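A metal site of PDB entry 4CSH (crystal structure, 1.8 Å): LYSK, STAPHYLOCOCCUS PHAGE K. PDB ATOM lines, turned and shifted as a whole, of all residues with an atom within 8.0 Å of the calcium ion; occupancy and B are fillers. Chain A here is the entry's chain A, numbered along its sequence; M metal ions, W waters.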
ATOM      1  N   TYR A  32      -3.004  15.630  26.427  1.00  0.00           N
ATOM      2  CA  TYR A  32      -4.416  15.532  26.617  1.00  0.00           C
ATOM      3  C   TYR A  32      -5.168  15.181  25.312  1.00  0.00           C
ATOM      4  O   TYR A  32      -6.325  14.805  25.374  1.00  0.00           O
ATOM      5  CB  TYR A  32      -4.994  16.814  27.204  1.00  0.00           C
ATOM      6  CG  TYR A  32      -4.696  18.123  26.431  1.00  0.00           C
ATOM      7  CD1 TYR A  32      -5.457  18.485  25.326  1.00  0.00           C
ATOM      8  CD2 TYR A  32      -3.741  19.011  26.868  1.00  0.00           C
ATOM      9  CE1 TYR A  32      -5.199  19.684  24.633  1.00  0.00           C
ATOM     10  CE2 TYR A  32      -3.452  20.218  26.171  1.00  0.00           C
ATOM     11  CZ  TYR A  32      -4.234  20.571  25.088  1.00  0.00           C
ATOM     12  OH  TYR A  32      -4.006  21.747  24.364  1.00  0.00           O
ATOM     13  N   MET A  39       3.370  16.968  24.290  1.00  0.00           N
ATOM     14  CA  MET A  39       4.096  18.254  24.231  1.00  0.00           C
ATOM     15  C   MET A  39       5.359  18.208  25.110  1.00  0.00           C
ATOM     16  O   MET A  39       5.288  17.963  26.313  1.00  0.00           O
ATOM     17  CB  MET A  39       3.226  19.421  24.712  1.00  0.00           C
ATOM     18  CG  MET A  39       2.010  19.703  23.858  1.00  0.00           C
ATOM     19  SD  MET A  39       1.159  21.204  24.376  1.00  0.00           S
ATOM     20  CE  MET A  39       0.268  20.647  25.854  1.00  0.00           C
ATOM     21  N   ILE A  44       4.655  25.829  23.841  1.00  0.00           N
ATOM     22  CA  ILE A  44       3.753  26.892  24.276  1.00  0.00           C
ATOM     23  C   ILE A  44       2.328  26.499  23.922  1.00  0.00           C
ATOM     24  O   ILE A  44       1.988  26.225  22.749  1.00  0.00           O
ATOM     25  CB  ILE A  44       4.119  28.231  23.593  1.00  0.00           C
ATOM     26  CG1 ILE A  44       5.602  28.610  23.769  1.00  0.00           C
ATOM     27  CG2 ILE A  44       3.176  29.346  24.030  1.00  0.00           C
ATOM     28  CD1 ILE A  44       6.095  28.727  25.191  1.00  0.00           C
ATOM     29  N   ASP A  45       1.468  26.418  24.944  1.00  0.00           N
ATOM     30  CA  ASP A  45       0.053  26.104  24.737  1.00  0.00           C
ATOM     31  C   ASP A  45      -0.745  27.159  25.501  1.00  0.00           C
ATOM     32  O   ASP A  45      -0.831  27.140  26.715  1.00  0.00           O
ATOM     33  CB  ASP A  45      -0.280  24.682  25.240  1.00  0.00           C
ATOM     34  CG  ASP A  45      -1.709  24.228  24.929  1.00  0.00           C
ATOM     35  OD1 ASP A  45      -2.415  24.900  24.133  1.00  0.00           O
ATOM     36  OD2 ASP A  45      -2.136  23.196  25.517  1.00  0.00           O
ATOM     37  N   ALA A  46      -1.329  28.066  24.737  1.00  0.00           N
ATOM     38  CA  ALA A  46      -1.988  29.248  25.303  1.00  0.00           C
ATOM     39  C   ALA A  46      -3.482  29.087  25.496  1.00  0.00           C
ATOM     40  O   ALA A  46      -4.068  29.910  26.169  1.00  0.00           O
ATOM     41  CB  ALA A  46      -1.663  30.474  24.453  1.00  0.00           C
ATOM     42  N   ASP A  47      -4.086  28.102  24.827  1.00  0.00           N
ATOM     43  CA  ASP A  47      -5.577  27.946  24.839  1.00  0.00           C
ATOM     44  C   ASP A  47      -6.081  26.662  25.495  1.00  0.00           C
ATOM     45  O   ASP A  47      -7.279  26.557  25.833  1.00  0.00           O
ATOM     46  CB  ASP A  47      -6.137  28.118  23.415  1.00  0.00           C
ATOM     47  CG  ASP A  47      -5.731  27.040  22.480  1.00  0.00           C
ATOM     48  OD1 ASP A  47      -4.815  26.230  22.798  1.00  0.00           O
ATOM     49  OD2 ASP A  47      -6.307  26.953  21.385  1.00  0.00           O
ATOM     50  N   GLY A  48      -5.194  25.696  25.716  1.00  0.00           N
ATOM     51  CA  GLY A  48      -5.591  24.400  26.249  1.00  0.00           C
ATOM     52  C   GLY A  48      -6.313  23.456  25.272  1.00  0.00           C
ATOM     53  O   GLY A  48      -6.869  22.457  25.692  1.00  0.00           O
ATOM     54  N   TYR A  49      -6.297  23.749  23.965  1.00  0.00           N
ATOM     55  CA  TYR A  49      -6.750  22.894  22.935  1.00  0.00           C
ATOM     56  C   TYR A  49      -5.647  22.580  21.941  1.00  0.00           C
ATOM     57  O   TYR A  49      -4.724  23.393  21.758  1.00  0.00           O
ATOM     58  CB  TYR A  49      -7.871  23.570  22.126  1.00  0.00           C
ATOM     59  CG  TYR A  49      -9.167  23.790  22.875  1.00  0.00           C
ATOM     60  CD1 TYR A  49      -9.999  22.741  23.197  1.00  0.00           C
ATOM     61  CD2 TYR A  49      -9.565  25.073  23.212  1.00  0.00           C
ATOM     62  CE1 TYR A  49     -11.178  22.963  23.874  1.00  0.00           C
ATOM     63  CE2 TYR A  49     -10.747  25.303  23.891  1.00  0.00           C
ATOM     64  CZ  TYR A  49     -11.545  24.253  24.207  1.00  0.00           C
ATOM     65  OH  TYR A  49     -12.742  24.469  24.893  1.00  0.00           O
ATOM     66  N   TYR A  50      -5.720  21.400  21.335  1.00  0.00           N
ATOM     67  CA  TYR A  50      -4.868  21.053  20.186  1.00  0.00           C
ATOM     68  C   TYR A  50      -3.344  21.019  20.437  1.00  0.00           C
ATOM     69  O   TYR A  50      -2.558  21.054  19.449  1.00  0.00           O
ATOM     70  CB  TYR A  50      -5.118  21.988  18.959  1.00  0.00           C
ATOM     71  CG  TYR A  50      -6.564  22.255  18.695  1.00  0.00           C
ATOM     72  CD1 TYR A  50      -7.439  21.214  18.387  1.00  0.00           C
ATOM     73  CD2 TYR A  50      -7.068  23.560  18.784  1.00  0.00           C
ATOM     74  CE1 TYR A  50      -8.805  21.464  18.205  1.00  0.00           C
ATOM     75  CE2 TYR A  50      -8.410  23.828  18.591  1.00  0.00           C
ATOM     76  CZ  TYR A  50      -9.289  22.784  18.296  1.00  0.00           C
ATOM     77  OH  TYR A  50     -10.629  23.075  18.148  1.00  0.00           O
ATOM     78  N   HIS A  51      -2.929  20.868  21.677  1.00  0.00           N
ATOM     79  CA  HIS A  51      -1.490  20.886  22.032  1.00  0.00           C
ATOM     80  C   HIS A  51      -0.822  22.186  21.507  1.00  0.00           C
ATOM     81  O   HIS A  51      -1.454  23.245  21.611  1.00  0.00           O
ATOM     82  CB  HIS A  51      -0.806  19.593  21.581  1.00  0.00           C
ATOM     83  CG  HIS A  51      -1.134  18.382  22.410  1.00  0.00           C
ATOM     84  ND1 HIS A  51      -0.378  17.225  22.371  1.00  0.00           N
ATOM     85  CD2 HIS A  51      -2.120  18.152  23.329  1.00  0.00           C
ATOM     86  CE1 HIS A  51      -0.890  16.332  23.215  1.00  0.00           C
ATOM     87  NE2 HIS A  51      -1.934  16.868  23.799  1.00  0.00           N
ATOM     88  N   ALA A  52       0.373  22.118  20.922  1.00  0.00           N
ATOM     89  CA  ALA A  52       1.171  23.329  20.696  1.00  0.00           C
ATOM     90  C   ALA A  52       1.179  23.633  19.214  1.00  0.00           C
ATOM     91  O   ALA A  52       1.993  23.110  18.434  1.00  0.00           O
ATOM     92  CB  ALA A  52       2.589  23.155  21.251  1.00  0.00           C
ATOM     93  N   GLN A  53       0.227  24.466  18.837  1.00  0.00           N
ATOM     94  CA  GLN A  53      -0.016  24.897  17.459  1.00  0.00           C
ATOM     95  C   GLN A  53       0.788  26.150  17.131  1.00  0.00           C
ATOM     96  O   GLN A  53       1.328  26.833  18.027  1.00  0.00           O
ATOM     97  CB  GLN A  53      -1.534  25.132  17.264  1.00  0.00           C
ATOM     98  CG  GLN A  53      -2.401  23.883  17.490  1.00  0.00           C
ATOM     99  CD  GLN A  53      -2.405  22.916  16.321  1.00  0.00           C
ATOM    100  OE1 GLN A  53      -2.427  23.354  15.135  1.00  0.00           O
ATOM    101  NE2 GLN A  53      -2.385  21.634  16.618  1.00  0.00           N
ATOM    102  N   CYS A  54       0.781  26.516  15.853  1.00  0.00           N
ATOM    103  CA  CYS A  54       1.520  27.669  15.417  1.00  0.00           C
ATOM    104  C   CYS A  54       0.983  28.950  16.062  1.00  0.00           C
ATOM    105  O   CYS A  54       1.763  29.761  16.562  1.00  0.00           O
ATOM    106  CB  CYS A  54       1.533  27.754  13.885  1.00  0.00           C
ATOM    107  SG  CYS A  54      -0.085  28.016  13.055  1.00  0.00           S
ATOM    108  N   GLN A  55      -0.349  29.095  16.137  1.00  0.00           N
ATOM    109  CA  GLN A  55      -0.928  30.331  16.688  1.00  0.00           C
ATOM    110  C   GLN A  55      -0.679  30.491  18.215  1.00  0.00           C
ATOM    111  O   GLN A  55      -0.580  31.615  18.714  1.00  0.00           O
ATOM    112  CB  GLN A  55      -2.408  30.456  16.353  1.00  0.00           C
ATOM    113  CG  GLN A  55      -3.042  31.747  16.880  1.00  0.00           C
ATOM    114  CD  GLN A  55      -2.470  32.994  16.288  1.00  0.00           C
ATOM    115  OE1 GLN A  55      -1.970  32.971  15.174  1.00  0.00           O
ATOM    116  NE2 GLN A  55      -2.505  34.077  17.033  1.00  0.00           N
ATOM    117  N   ASP A  56      -0.540  29.393  18.959  1.00  0.00           N
ATOM    118  CA  ASP A  56      -0.195  29.436  20.406  1.00  0.00           C
ATOM    119  C   ASP A  56       1.038  30.333  20.724  1.00  0.00           C
ATOM    120  O   ASP A  56       1.028  31.170  21.631  1.00  0.00           O
ATOM    121  CB  ASP A  56       0.110  28.023  20.931  1.00  0.00           C
ATOM    122  CG  ASP A  56      -1.123  27.188  21.203  1.00  0.00           C
ATOM    123  OD1 ASP A  56      -2.021  27.567  21.972  1.00  0.00           O
ATOM    124  OD2 ASP A  56      -1.204  26.034  20.671  1.00  0.00           O
ATOM    125  N   LEU A  57       2.103  30.196  19.897  1.00  0.00           N
ATOM    126  CA  LEU A  57       3.277  31.005  20.058  1.00  0.00           C
ATOM    127  C   LEU A  57       2.919  32.471  19.937  1.00  0.00           C
ATOM    128  O   LEU A  57       3.410  33.310  20.677  1.00  0.00           O
ATOM    129  CB  LEU A  57       4.329  30.630  18.986  1.00  0.00           C
ATOM    130  CG  LEU A  57       5.620  31.429  18.974  1.00  0.00           C
ATOM    131  CD1 LEU A  57       6.312  31.396  20.339  1.00  0.00           C
ATOM    132  CD2 LEU A  57       6.576  30.934  17.908  1.00  0.00           C
ATOM    133  N   GLN A 135       5.980  27.310  15.883  1.00  0.00           N
ATOM    134  CA  GLN A 135       5.511  25.997  16.305  1.00  0.00           C
ATOM    135  C   GLN A 135       4.762  25.228  15.207  1.00  0.00           C
ATOM    136  O   GLN A 135       4.138  25.785  14.304  1.00  0.00           O
ATOM    137  CB  GLN A 135       4.623  26.125  17.558  1.00  0.00           C
ATOM    138  CG  GLN A 135       5.500  26.344  18.789  1.00  0.00           C
ATOM    139  CD  GLN A 135       4.768  26.261  20.140  1.00  0.00           C
ATOM    140  OE1 GLN A 135       5.429  26.164  21.157  1.00  0.00           O
ATOM    141  NE2 GLN A 135       3.439  26.399  20.145  1.00  0.00           N
ATOM    142  N   ALA A 141       2.184  18.961  16.667  1.00  0.00           N
ATOM    143  CA  ALA A 141       1.891  19.923  17.750  1.00  0.00           C
ATOM    144  C   ALA A 141       2.597  19.578  19.065  1.00  0.00           C
ATOM    145  O   ALA A 141       2.105  19.871  20.149  1.00  0.00           O
ATOM    146  CB  ALA A 141       0.388  20.040  17.956  1.00  0.00           C
HETATM  147 CA    CA M   1      -3.022  25.073  21.899  1.00  0.00          CA
HETATM  148  O   HOH W   1      -4.213  25.914  19.899  1.00  0.00           O
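The side-chain carboxylate of Asp 45 sits at hydrogen-bond distance from the side-chain hydroxyl of Tyr 32, at 2.6 Å. The backbone NH (N) of His 51 sits at hydrogen-bond distance from the side-chain hydroxyl (OH) of Tyr 32 (3.0 Å). The backbone NH of Gly 48 sits close to the side-chain carboxylate of Asp 45, at 3.3 Å. The side-chain hydroxyl (OH) of Tyr 32 sits close to the backbone NH (N) of Tyr 49 (3.1 Å). The backbone NH (N) of Gln 53 lies close to the side-chain carboxylate (OD2) of Asp 56, at 2.8 Å. The backbone NH of Ala 46 lies close to the side-chain carboxylate of Asp 56.
Of the 18 residues printed, 5 come within 4 Å of the calcium ion.
The calcium ion is bound by the side-chain carboxylate (OD1) of Asp 47 (2.3 Å), the side-chain carboxylate (OD1) of Asp 45 (2.3 Å), the side-chain carboxylate (OD2) of Asp 56 (2.4 Å), the backbone carbonyl oxygen (O) of Tyr 49 (2.4 Å), the backbone carbonyl oxygen (O) of His 51 (2.4 Å), water W1 (2.5 Å) and the side-chain carboxylate (OD1) of Asp 56 (2.7 Å). The calcium ion has seven donor atoms within binding distance.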
